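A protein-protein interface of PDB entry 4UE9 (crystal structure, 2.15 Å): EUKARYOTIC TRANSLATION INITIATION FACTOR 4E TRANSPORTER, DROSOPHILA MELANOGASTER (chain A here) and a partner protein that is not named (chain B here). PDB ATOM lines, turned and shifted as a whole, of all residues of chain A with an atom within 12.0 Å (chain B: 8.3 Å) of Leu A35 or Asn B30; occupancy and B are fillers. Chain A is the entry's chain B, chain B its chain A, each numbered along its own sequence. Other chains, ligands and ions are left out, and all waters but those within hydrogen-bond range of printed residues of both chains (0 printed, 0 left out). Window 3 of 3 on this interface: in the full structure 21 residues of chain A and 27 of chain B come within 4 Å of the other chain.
N of Gly A36 sits at hydrogen-bond distance from OE1 of Glu B18 (3.4 Å). The backbone NH (N) of Lys B49 is in hydrogen-bond range of the backbone carbonyl oxygen (O) of Phe A37, at 2.8 Å. The side-chain amino group of Lys B49 sits at hydrogen-bond distance from the backbone carbonyl oxygen of Gly A36, at 3.0 Å.
Of the printed residues of chain B, Arg A29 touches Ile B32 (3.9 Å) and Thr B33 (3.3 Å). Leu A35 touches one residue of chain B. Of the printed residues of chain B, Trp A38 touches Lys B49 (3.5 Å). No residue of chain A comes within 4 Å of Leu B14. No residue of chain A comes within 4 Å of Leu B17. Printed residues of chain A within 4 Å of Glu B18: Gly A36 (3.4 Å). No residue of chain A comes within 4 Å of Gln B29. Asn B30 touches just one residue of chain A: Leu A35 (3.7 Å). No residue of chain A comes within 4 Å of Glu B31. Printed residues of chain A within 4 Å of Lys B49: Gly A36, Phe A37 and Trp A38. Asp B59 touches none of the printed residues of chain A. Of the printed residues of chain A, Tyr B60 touches Phe A37. No residue of chain A comes within 4 Å of Ser B61. The nearest printed residue of chain B that does not touch Trp A38 is Ile B32 (4.4 Å).
The side-chain hydroxyl (OH) of Tyr B60 lies within hydrogen-bond range of the backbone carbonyl oxygen (O) of Lys B49, at 2.8 Å. N of Tyr B16 sits at hydrogen-bond distance from O of Asn B30 (2.8 Å). The side-chain amide nitrogen (ND2) of Asn B30 lies within hydrogen-bond range of the backbone carbonyl oxygen (O) of Met B28 (3.1 Å). The backbone NH (N) of Leu B14 lies within hydrogen-bond range of the backbone carbonyl oxygen (O) of Thr B33, 2.9 Å away. OH of Tyr B16 lies within hydrogen-bond range of OG of Ser B58 (3.4 Å). The side-chain hydroxyl of Tyr B16 lies within hydrogen-bond range of the side-chain carboxylate of Glu B18.
O of Ile B32 touches CB of Arg A29, 3.9 Å away. Thr B33 touches Arg A29 (OG1 to CB, 3.3 Å). CD1 of Leu A35 touches CG of Asn B30, at 3.7 Å. Tyr B16 touches Phe A37 (CD2 to CD1, 3.5 Å). CD1 of Ile B32 touches CZ of Phe A37, at 3.5 Å. CB of Phe A37 touches OH of Tyr B60, at 3.5 Å. Trp A38 touches Lys B49 (O to CE, 3.5 Å).
Of the 23 printed residues of chain B, 7 touch a printed residue of chain A. Printed residues of chain B that touch a printed residue of chain A: Tyr B16, Glu B18, Asn B30, Ile B32, Thr B33, Lys B49 and Tyr B60. Hydrophobic or aromatic side chains of chain A that line the printed part of chain B: Leu A35 and Phe A37. Among the printed residues, 10 pairs touch across the chains. Among the printed residues, no Asp or Glu carboxylate lies within 4 Å of a Lys or Arg side-chain nitrogen of the other chain.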
ATOM      1  N   ARG A  29      32.701  28.481  30.786  1.00  0.00           N
ATOM      2  CA  ARG A  29      31.647  28.571  29.782  1.00  0.00           C
ATOM      3  C   ARG A  29      30.271  28.740  30.417  1.00  0.00           C
ATOM      4  O   ARG A  29      29.734  27.808  31.017  1.00  0.00           O
ATOM      5  CB  ARG A  29      31.660  27.331  28.887  1.00  0.00           C
ATOM      6  N   LEU A  30      29.712  29.939  30.278  1.00  0.00           N
ATOM      7  CA  LEU A  30      28.371  30.239  30.769  1.00  0.00           C
ATOM      8  C   LEU A  30      27.621  31.085  29.740  1.00  0.00           C
ATOM      9  O   LEU A  30      27.410  32.280  29.934  1.00  0.00           O
ATOM     10  CB  LEU A  30      28.444  30.962  32.118  1.00  0.00           C
ATOM     11  CG  LEU A  30      27.117  31.331  32.788  1.00  0.00           C
ATOM     12  CD1 LEU A  30      26.252  30.100  33.020  1.00  0.00           C
ATOM     13  CD2 LEU A  30      27.374  32.058  34.098  1.00  0.00           C
ATOM     14  N   GLU A  31      27.231  30.453  28.637  1.00  0.00           N
ATOM     15  CA  GLU A  31      26.511  31.135  27.565  1.00  0.00           C
ATOM     16  C   GLU A  31      25.118  31.543  28.017  1.00  0.00           C
ATOM     17  O   GLU A  31      24.584  30.992  28.980  1.00  0.00           O
ATOM     18  CB  GLU A  31      26.407  30.235  26.331  1.00  0.00           C
ATOM     19  CG  GLU A  31      27.738  29.917  25.673  1.00  0.00           C
ATOM     20  CD  GLU A  31      27.590  29.016  24.461  1.00  0.00           C
ATOM     21  OE1 GLU A  31      26.703  28.135  24.477  1.00  0.00           O
ATOM     22  OE2 GLU A  31      28.365  29.184  23.495  1.00  0.00           O
ATOM     23  N   LEU A  32      24.527  32.509  27.321  1.00  0.00           N
ATOM     24  CA  LEU A  32      23.158  32.910  27.612  1.00  0.00           C
ATOM     25  C   LEU A  32      22.198  31.782  27.243  1.00  0.00           C
ATOM     26  O   LEU A  32      21.489  31.847  26.238  1.00  0.00           O
ATOM     27  CB  LEU A  32      22.797  34.202  26.869  1.00  0.00           C
ATOM     28  CG  LEU A  32      23.213  35.506  27.560  1.00  0.00           C
ATOM     29  CD1 LEU A  32      23.014  36.695  26.633  1.00  0.00           C
ATOM     30  CD2 LEU A  32      22.430  35.709  28.852  1.00  0.00           C
ATOM     31  N   GLN A  33      22.210  30.739  28.066  1.00  0.00           N
ATOM     32  CA  GLN A  33      21.295  29.612  27.931  1.00  0.00           C
ATOM     33  C   GLN A  33      20.663  29.326  29.289  1.00  0.00           C
ATOM     34  O   GLN A  33      21.367  29.139  30.282  1.00  0.00           O
ATOM     35  CB  GLN A  33      22.027  28.376  27.401  1.00  0.00           C
ATOM     36  CG  GLN A  33      23.105  27.839  28.335  1.00  0.00           C
ATOM     37  CD  GLN A  33      24.004  26.819  27.665  1.00  0.00           C
ATOM     38  OE1 GLN A  33      23.606  26.159  26.707  1.00  0.00           O
ATOM     39  NE2 GLN A  33      25.228  26.693  28.163  1.00  0.00           N
ATOM     40  N   THR A  34      19.334  29.312  29.333  1.00  0.00           N
ATOM     41  CA  THR A  34      18.616  29.073  30.579  1.00  0.00           C
ATOM     42  C   THR A  34      18.144  27.626  30.642  1.00  0.00           C
ATOM     43  O   THR A  34      17.169  27.249  29.991  1.00  0.00           O
ATOM     44  CB  THR A  34      17.409  30.009  30.732  1.00  0.00           C
ATOM     45  OG1 THR A  34      17.810  31.357  30.462  1.00  0.00           O
ATOM     46  CG2 THR A  34      16.843  29.923  32.143  1.00  0.00           C
ATOM     47  N   LEU A  35      18.849  26.822  31.430  1.00  0.00           N
ATOM     48  CA  LEU A  35      18.546  25.404  31.561  1.00  0.00           C
ATOM     49  C   LEU A  35      18.591  25.003  33.031  1.00  0.00           C
ATOM     50  O   LEU A  35      19.251  25.655  33.840  1.00  0.00           O
ATOM     51  CB  LEU A  35      19.527  24.573  30.733  1.00  0.00           C
ATOM     52  CG  LEU A  35      19.470  24.829  29.223  1.00  0.00           C
ATOM     53  CD1 LEU A  35      20.689  24.246  28.529  1.00  0.00           C
ATOM     54  CD2 LEU A  35      18.191  24.258  28.628  1.00  0.00           C
ATOM     55  N   GLY A  36      17.886  23.929  33.372  1.00  0.00           N
ATOM     56  CA  GLY A  36      17.701  23.554  34.760  1.00  0.00           C
ATOM     57  C   GLY A  36      18.826  22.739  35.369  1.00  0.00           C
ATOM     58  O   GLY A  36      18.737  22.346  36.529  1.00  0.00           O
ATOM     59  N   PHE A  37      19.886  22.488  34.606  1.00  0.00           N
ATOM     60  CA  PHE A  37      20.967  21.632  35.090  1.00  0.00           C
ATOM     61  C   PHE A  37      21.923  22.391  36.004  1.00  0.00           C
ATOM     62  O   PHE A  37      22.620  21.785  36.819  1.00  0.00           O
ATOM     63  CB  PHE A  37      21.741  21.024  33.918  1.00  0.00           C
ATOM     64  CG  PHE A  37      22.671  21.980  33.235  1.00  0.00           C
ATOM     65  CD1 PHE A  37      22.231  22.758  32.179  1.00  0.00           C
ATOM     66  CD2 PHE A  37      23.990  22.093  33.641  1.00  0.00           C
ATOM     67  CE1 PHE A  37      23.088  23.637  31.547  1.00  0.00           C
ATOM     68  CE2 PHE A  37      24.849  22.969  33.013  1.00  0.00           C
ATOM     69  CZ  PHE A  37      24.398  23.741  31.965  1.00  0.00           C
ATOM     70  N   TRP A  38      21.956  23.712  35.865  1.00  0.00           N
ATOM     71  CA  TRP A  38      22.822  24.541  36.696  1.00  0.00           C
ATOM     72  C   TRP A  38      22.439  24.438  38.167  1.00  0.00           C
ATOM     73  O   TRP A  38      21.263  24.508  38.518  1.00  0.00           O
ATOM     74  CB  TRP A  38      22.766  26.003  36.251  1.00  0.00           C
ATOM     75  CG  TRP A  38      23.528  26.287  34.995  1.00  0.00           C
ATOM     76  CD1 TRP A  38      23.028  26.784  33.825  1.00  0.00           C
ATOM     77  CD2 TRP A  38      24.931  26.094  34.780  1.00  0.00           C
ATOM     78  NE1 TRP A  38      24.032  26.913  32.897  1.00  0.00           N
ATOM     79  CE2 TRP A  38      25.211  26.498  33.458  1.00  0.00           C
ATOM     80  CE3 TRP A  38      25.979  25.623  35.578  1.00  0.00           C
ATOM     81  CZ2 TRP A  38      26.493  26.438  32.916  1.00  0.00           C
ATOM     82  CZ3 TRP A  38      27.251  25.567  35.037  1.00  0.00           C
ATOM     83  CH2 TRP A  38      27.498  25.972  33.720  1.00  0.00           C
ATOM     84  N   LYS A  39      23.443  24.272  39.020  1.00  0.00           N
ATOM     85  CA  LYS A  39      23.226  24.185  40.457  1.00  0.00           C
ATOM     86  C   LYS A  39      22.948  25.569  41.035  1.00  0.00           C
ATOM     87  O   LYS A  39      23.320  26.583  40.441  1.00  0.00           O
ATOM     88  CB  LYS A  39      24.443  23.555  41.138  1.00  0.00           C
ATOM     89  CG  LYS A  39      24.234  23.210  42.607  1.00  0.00           C
ATOM     90  CD  LYS A  39      25.497  22.641  43.242  1.00  0.00           C
ATOM     91  CE  LYS A  39      25.885  21.303  42.635  1.00  0.00           C
ATOM     92  NZ  LYS A  39      27.049  20.693  43.337  1.00  0.00           N
ATOM     93  N   ILE A  40      22.284  25.604  42.187  1.00  0.00           N
ATOM     94  CA  ILE A  40      21.995  26.858  42.874  1.00  0.00           C
ATOM     95  C   ILE A  40      22.227  26.703  44.375  1.00  0.00           C
ATOM     96  O   ILE A  40      22.111  25.607  44.926  1.00  0.00           O
ATOM     97  CB  ILE A  40      20.542  27.326  42.614  1.00  0.00           C
ATOM     98  CG1 ILE A  40      20.300  28.718  43.210  1.00  0.00           C
ATOM     99  CG2 ILE A  40      19.538  26.316  43.170  1.00  0.00           C
ATOM    100  CD1 ILE A  40      21.073  29.833  42.520  1.00  0.00           C
ATOM    101  OXT ILE A  40      22.538  27.671  45.070  1.00  0.00           O
ATOM    102  N   THR B  13      33.822  16.724  26.493  1.00  0.00           N
ATOM    103  CA  THR B  13      32.738  17.691  26.363  1.00  0.00           C
ATOM    104  C   THR B  13      31.488  17.192  27.079  1.00  0.00           C
ATOM    105  O   THR B  13      31.023  16.074  26.835  1.00  0.00           O
ATOM    106  CB  THR B  13      32.404  17.965  24.883  1.00  0.00           C
ATOM    107  OG1 THR B  13      33.568  18.467  24.215  1.00  0.00           O
ATOM    108  CG2 THR B  13      31.274  18.979  24.751  1.00  0.00           C
ATOM    109  N   LEU B  14      30.956  18.025  27.968  1.00  0.00           N
ATOM    110  CA  LEU B  14      29.703  17.734  28.648  1.00  0.00           C
ATOM    111  C   LEU B  14      28.525  18.252  27.834  1.00  0.00           C
ATOM    112  O   LEU B  14      28.504  19.416  27.420  1.00  0.00           O
ATOM    113  CB  LEU B  14      29.685  18.356  30.047  1.00  0.00           C
ATOM    114  CG  LEU B  14      28.386  18.163  30.840  1.00  0.00           C
ATOM    115  CD1 LEU B  14      28.179  16.703  31.206  1.00  0.00           C
ATOM    116  CD2 LEU B  14      28.377  19.031  32.086  1.00  0.00           C
ATOM    117  N   TRP B  15      27.550  17.377  27.612  1.00  0.00           N
ATOM    118  CA  TRP B  15      26.308  17.739  26.944  1.00  0.00           C
ATOM    119  C   TRP B  15      25.145  17.583  27.915  1.00  0.00           C
ATOM    120  O   TRP B  15      25.215  16.788  28.855  1.00  0.00           O
ATOM    121  CB  TRP B  15      26.071  16.870  25.710  1.00  0.00           C
ATOM    122  CG  TRP B  15      27.163  16.923  24.688  1.00  0.00           C
ATOM    123  CD1 TRP B  15      28.407  16.372  24.785  1.00  0.00           C
ATOM    124  CD2 TRP B  15      27.099  17.548  23.400  1.00  0.00           C
ATOM    125  NE1 TRP B  15      29.125  16.622  23.640  1.00  0.00           N
ATOM    126  CE2 TRP B  15      28.346  17.343  22.775  1.00  0.00           C
ATOM    127  CE3 TRP B  15      26.112  18.264  22.718  1.00  0.00           C
ATOM    128  CZ2 TRP B  15      28.628  17.825  21.499  1.00  0.00           C
ATOM    129  CZ3 TRP B  15      26.394  18.744  21.452  1.00  0.00           C
ATOM    130  CH2 TRP B  15      27.642  18.525  20.856  1.00  0.00           C
ATOM    131  N   TYR B  16      24.077  18.338  27.681  1.00  0.00           N
ATOM    132  CA  TYR B  16      22.872  18.240  28.499  1.00  0.00           C
ATOM    133  C   TYR B  16      21.628  18.284  27.622  1.00  0.00           C
ATOM    134  O   TYR B  16      21.385  19.265  26.922  1.00  0.00           O
ATOM    135  CB  TYR B  16      22.826  19.363  29.535  1.00  0.00           C
ATOM    136  CG  TYR B  16      21.544  19.404  30.335  1.00  0.00           C
ATOM    137  CD1 TYR B  16      21.245  18.409  31.259  1.00  0.00           C
ATOM    138  CD2 TYR B  16      20.635  20.439  30.171  1.00  0.00           C
ATOM    139  CE1 TYR B  16      20.074  18.444  31.994  1.00  0.00           C
ATOM    140  CE2 TYR B  16      19.464  20.484  30.901  1.00  0.00           C
ATOM    141  CZ  TYR B  16      19.186  19.484  31.809  1.00  0.00           C
ATOM    142  OH  TYR B  16      18.020  19.525  32.539  1.00  0.00           O
ATOM    143  N   LEU B  17      20.855  17.203  27.658  1.00  0.00           N
ATOM    144  CA  LEU B  17      19.603  17.114  26.918  1.00  0.00           C
ATOM    145  C   LEU B  17      18.443  17.511  27.820  1.00  0.00           C
ATOM    146  O   LEU B  17      18.352  17.055  28.957  1.00  0.00           O
ATOM    147  CB  LEU B  17      19.392  15.696  26.386  1.00  0.00           C
ATOM    148  CG  LEU B  17      18.127  15.438  25.562  1.00  0.00           C
ATOM    149  CD1 LEU B  17      18.338  15.838  24.112  1.00  0.00           C
ATOM    150  CD2 LEU B  17      17.715  13.980  25.663  1.00  0.00           C
ATOM    151  N   GLU B  18      17.563  18.367  27.311  1.00  0.00           N
ATOM    152  CA  GLU B  18      16.362  18.754  28.040  1.00  0.00           C
ATOM    153  C   GLU B  18      15.193  18.888  27.077  1.00  0.00           C
ATOM    154  O   GLU B  18      15.333  19.451  25.991  1.00  0.00           O
ATOM    155  CB  GLU B  18      16.583  20.063  28.799  1.00  0.00           C
ATOM    156  CG  GLU B  18      15.355  20.558  29.548  1.00  0.00           C
ATOM    157  CD  GLU B  18      15.667  21.696  30.499  1.00  0.00           C
ATOM    158  OE1 GLU B  18      16.627  21.569  31.290  1.00  0.00           O
ATOM    159  OE2 GLU B  18      14.947  22.715  30.464  1.00  0.00           O
ATOM    160  N   ASN B  19      14.042  18.358  27.475  1.00  0.00           N
ATOM    161  CA  ASN B  19      12.869  18.373  26.614  1.00  0.00           C
ATOM    162  C   ASN B  19      12.288  19.771  26.449  1.00  0.00           C
ATOM    163  O   ASN B  19      12.006  20.462  27.427  1.00  0.00           O
ATOM    164  CB  ASN B  19      11.805  17.418  27.152  1.00  0.00           C
ATOM    165  CG  ASN B  19      11.882  16.048  26.509  1.00  0.00           C
ATOM    166  OD1 ASN B  19      10.979  15.641  25.778  1.00  0.00           O
ATOM    167  ND2 ASN B  19      12.975  15.335  26.761  1.00  0.00           N
ATOM    168  N   ASP B  20      12.118  20.171  25.193  1.00  0.00           N
ATOM    169  CA  ASP B  20      11.639  21.502  24.848  1.00  0.00           C
ATOM    170  C   ASP B  20      10.909  21.453  23.510  1.00  0.00           C
ATOM    171  O   ASP B  20      11.098  20.520  22.728  1.00  0.00           O
ATOM    172  CB  ASP B  20      12.805  22.491  24.786  1.00  0.00           C
ATOM    173  CG  ASP B  20      12.358  23.905  24.475  1.00  0.00           C
ATOM    174  OD1 ASP B  20      12.186  24.226  23.280  1.00  0.00           O
ATOM    175  OD2 ASP B  20      12.181  24.697  25.425  1.00  0.00           O
ATOM    176  N   GLU B  26      16.308  17.640  17.287  1.00  0.00           N
ATOM    177  CA  GLU B  26      17.645  17.185  17.658  1.00  0.00           C
ATOM    178  C   GLU B  26      18.468  18.332  18.241  1.00  0.00           C
ATOM    179  O   GLU B  26      19.614  18.139  18.651  1.00  0.00           O
ATOM    180  CB  GLU B  26      18.373  16.575  16.453  1.00  0.00           C
ATOM    181  CG  GLU B  26      18.230  17.356  15.151  1.00  0.00           C
ATOM    182  CD  GLU B  26      16.934  17.056  14.409  1.00  0.00           C
ATOM    183  OE1 GLU B  26      16.157  16.194  14.873  1.00  0.00           O
ATOM    184  OE2 GLU B  26      16.696  17.688  13.358  1.00  0.00           O
ATOM    185  N   ASP B  27      17.876  19.523  18.276  1.00  0.00           N
ATOM    186  CA  ASP B  27      18.516  20.686  18.882  1.00  0.00           C
ATOM    187  C   ASP B  27      18.260  20.728  20.384  1.00  0.00           C
ATOM    188  O   ASP B  27      18.621  21.691  21.061  1.00  0.00           O
ATOM    189  CB  ASP B  27      18.012  21.970  18.226  1.00  0.00           C
ATOM    190  CG  ASP B  27      18.314  22.022  16.742  1.00  0.00           C
ATOM    191  OD1 ASP B  27      19.368  21.493  16.331  1.00  0.00           O
ATOM    192  OD2 ASP B  27      17.495  22.587  15.986  1.00  0.00           O
ATOM    193  N   MET B  28      17.631  19.677  20.897  1.00  0.00           N
ATOM    194  CA  MET B  28      17.338  19.571  22.318  1.00  0.00           C
ATOM    195  C   MET B  28      18.612  19.245  23.092  1.00  0.00           C
ATOM    196  O   MET B  28      18.668  19.392  24.315  1.00  0.00           O
ATOM    197  CB  MET B  28      16.272  18.498  22.558  1.00  0.00           C
ATOM    198  CG  MET B  28      15.044  18.639  21.660  1.00  0.00           C
ATOM    199  SD  MET B  28      13.976  17.188  21.663  1.00  0.00           S
ATOM    200  CE  MET B  28      13.333  17.252  23.326  1.00  0.00           C
ATOM    201  N   GLN B  29      19.633  18.799  22.365  1.00  0.00           N
ATOM    202  CA  GLN B  29      20.935  18.501  22.946  1.00  0.00           C
ATOM    203  C   GLN B  29      21.782  19.772  23.021  1.00  0.00           C
ATOM    204  O   GLN B  29      21.974  20.455  22.014  1.00  0.00           O
ATOM    205  CB  GLN B  29      21.647  17.428  22.118  1.00  0.00           C
ATOM    206  CG  GLN B  29      22.848  16.799  22.800  1.00  0.00           C
ATOM    207  CD  GLN B  29      22.467  15.963  24.004  1.00  0.00           C
ATOM    208  OE1 GLN B  29      22.525  16.430  25.140  1.00  0.00           O
ATOM    209  NE2 GLN B  29      22.075  14.718  23.761  1.00  0.00           N
ATOM    210  N   ASN B  30      22.279  20.079  24.216  1.00  0.00           N
ATOM    211  CA  ASN B  30      23.050  21.298  24.448  1.00  0.00           C
ATOM    212  C   ASN B  30      24.503  21.010  24.806  1.00  0.00           C
ATOM    213  O   ASN B  30      24.780  20.326  25.788  1.00  0.00           O
ATOM    214  CB  ASN B  30      22.409  22.124  25.567  1.00  0.00           C
ATOM    215  CG  ASN B  30      20.952  22.445  25.298  1.00  0.00           C
ATOM    216  OD1 ASN B  30      20.634  23.412  24.605  1.00  0.00           O
ATOM    217  ND2 ASN B  30      20.056  21.636  25.852  1.00  0.00           N
ATOM    218  N   GLU B  31      25.427  21.541  24.009  1.00  0.00           N
ATOM    219  CA  GLU B  31      26.850  21.457  24.321  1.00  0.00           C
ATOM    220  C   GLU B  31      27.208  22.482  25.389  1.00  0.00           C
ATOM    221  O   GLU B  31      27.281  23.679  25.111  1.00  0.00           O
ATOM    222  CB  GLU B  31      27.695  21.685  23.066  1.00  0.00           C
ATOM    223  CG  GLU B  31      29.196  21.643  23.314  1.00  0.00           C
ATOM    224  CD  GLU B  31      30.001  21.759  22.036  1.00  0.00           C
ATOM    225  OE1 GLU B  31      29.394  21.957  20.962  1.00  0.00           O
ATOM    226  OE2 GLU B  31      31.244  21.653  22.105  1.00  0.00           O
ATOM    227  N   ILE B  32      27.431  22.013  26.611  1.00  0.00           N
ATOM    228  CA  ILE B  32      27.710  22.907  27.728  1.00  0.00           C
ATOM    229  C   ILE B  32      29.123  23.471  27.639  1.00  0.00           C
ATOM    230  O   ILE B  32      29.305  24.662  27.385  1.00  0.00           O
ATOM    231  CB  ILE B  32      27.524  22.190  29.079  1.00  0.00           C
ATOM    232  CG1 ILE B  32      26.155  21.501  29.127  1.00  0.00           C
ATOM    233  CG2 ILE B  32      27.667  23.170  30.238  1.00  0.00           C
ATOM    234  CD1 ILE B  32      24.986  22.406  28.759  1.00  0.00           C
ATOM    235  N   THR B  33      30.124  22.621  27.842  1.00  0.00           N
ATOM    236  CA  THR B  33      31.510  23.068  27.789  1.00  0.00           C
ATOM    237  C   THR B  33      32.476  21.902  27.628  1.00  0.00           C
ATOM    238  O   THR B  33      32.080  20.736  27.708  1.00  0.00           O
ATOM    239  CB  THR B  33      31.889  23.859  29.058  1.00  0.00           C
ATOM    240  OG1 THR B  33      33.219  24.377  28.925  1.00  0.00           O
ATOM    241  CG2 THR B  33      31.807  22.975  30.300  1.00  0.00           C
ATOM    242  N   LYS B  49      23.902  20.190  38.754  1.00  0.00           N
ATOM    243  CA  LYS B  49      23.073  19.310  39.566  1.00  0.00           C
ATOM    244  C   LYS B  49      23.442  17.848  39.343  1.00  0.00           C
ATOM    245  O   LYS B  49      23.721  17.442  38.215  1.00  0.00           O
ATOM    246  CB  LYS B  49      21.592  19.519  39.247  1.00  0.00           C
ATOM    247  CG  LYS B  49      21.025  20.834  39.748  1.00  0.00           C
ATOM    248  CD  LYS B  49      19.561  20.973  39.375  1.00  0.00           C
ATOM    249  CE  LYS B  49      18.976  22.285  39.874  1.00  0.00           C
ATOM    250  NZ  LYS B  49      17.608  22.524  39.337  1.00  0.00           N
ATOM    251  N   LYS B  55      15.652  16.853  35.790  1.00  0.00           N
ATOM    252  CA  LYS B  55      14.267  16.707  35.360  1.00  0.00           C
ATOM    253  C   LYS B  55      14.083  15.427  34.553  1.00  0.00           C
ATOM    254  O   LYS B  55      15.015  14.950  33.905  1.00  0.00           O
ATOM    255  CB  LYS B  55      13.839  17.921  34.531  1.00  0.00           C
ATOM    256  CG  LYS B  55      12.345  17.994  34.240  1.00  0.00           C
ATOM    257  CD  LYS B  55      12.020  19.075  33.214  1.00  0.00           C
ATOM    258  CE  LYS B  55      12.264  20.479  33.752  1.00  0.00           C
ATOM    259  NZ  LYS B  55      11.331  20.829  34.859  1.00  0.00           N
ATOM    260  N   SER B  58      15.520  14.223  30.749  1.00  0.00           N
ATOM    261  CA  SER B  58      16.788  14.891  30.473  1.00  0.00           C
ATOM    262  C   SER B  58      17.966  13.922  30.558  1.00  0.00           C
ATOM    263  O   SER B  58      17.887  12.897  31.239  1.00  0.00           O
ATOM    264  CB  SER B  58      16.992  16.051  31.447  1.00  0.00           C
ATOM    265  OG  SER B  58      16.095  17.116  31.176  1.00  0.00           O
ATOM    266  N   ASP B  59      19.049  14.254  29.856  1.00  0.00           N
ATOM    267  CA  ASP B  59      20.277  13.459  29.872  1.00  0.00           C
ATOM    268  C   ASP B  59      21.509  14.294  30.198  1.00  0.00           C
ATOM    269  O   ASP B  59      21.575  15.475  29.870  1.00  0.00           O
ATOM    270  CB  ASP B  59      20.516  12.788  28.516  1.00  0.00           C
ATOM    271  CG  ASP B  59      19.359  11.928  28.069  1.00  0.00           C
ATOM    272  OD1 ASP B  59      18.566  11.492  28.927  1.00  0.00           O
ATOM    273  OD2 ASP B  59      19.253  11.674  26.850  1.00  0.00           O
ATOM    274  N   TYR B  60      22.479  13.657  30.846  1.00  0.00           N
ATOM    275  CA  TYR B  60      23.854  14.135  30.861  1.00  0.00           C
ATOM    276  C   TYR B  60      24.647  13.226  29.933  1.00  0.00           C
ATOM    277  O   TYR B  60      24.430  12.014  29.919  1.00  0.00           O
ATOM    278  CB  TYR B  60      24.461  14.098  32.265  1.00  0.00           C
ATOM    279  CG  TYR B  60      24.194  15.295  33.147  1.00  0.00           C
ATOM    280  CD1 TYR B  60      24.332  16.593  32.674  1.00  0.00           C
ATOM    281  CD2 TYR B  60      23.827  15.119  34.472  1.00  0.00           C
ATOM    282  CE1 TYR B  60      24.098  17.681  33.499  1.00  0.00           C
ATOM    283  CE2 TYR B  60      23.591  16.189  35.297  1.00  0.00           C
ATOM    284  CZ  TYR B  60      23.728  17.469  34.810  1.00  0.00           C
ATOM    285  OH  TYR B  60      23.489  18.532  35.647  1.00  0.00           O
ATOM    286  N   SER B  61      25.555  13.805  29.158  1.00  0.00           N
ATOM    287  CA  SER B  61      26.443  13.022  28.309  1.00  0.00           C
ATOM    288  C   SER B  61      27.838  13.615  28.335  1.00  0.00           C
ATOM    289  O   SER B  61      28.007  14.824  28.161  1.00  0.00           O
ATOM    290  CB  SER B  61      25.927  12.969  26.870  1.00  0.00           C
ATOM    291  OG  SER B  61      24.546  12.669  26.823  1.00  0.00           O
ATOM    292  N   PRO B  69      26.885  13.179  21.059  1.00  0.00           N
ATOM    293  CA  PRO B  69      26.252  12.106  21.836  1.00  0.00           C
ATOM    294  C   PRO B  69      25.098  11.439  21.085  1.00  0.00           C
ATOM    295  O   PRO B  69      23.989  11.315  21.605  1.00  0.00           O
ATOM    296  CB  PRO B  69      25.764  12.839  23.090  1.00  0.00           C
ATOM    297  CG  PRO B  69      25.476  14.209  22.621  1.00  0.00           C
ATOM    298  CD  PRO B  69      26.533  14.510  21.587  1.00  0.00           C
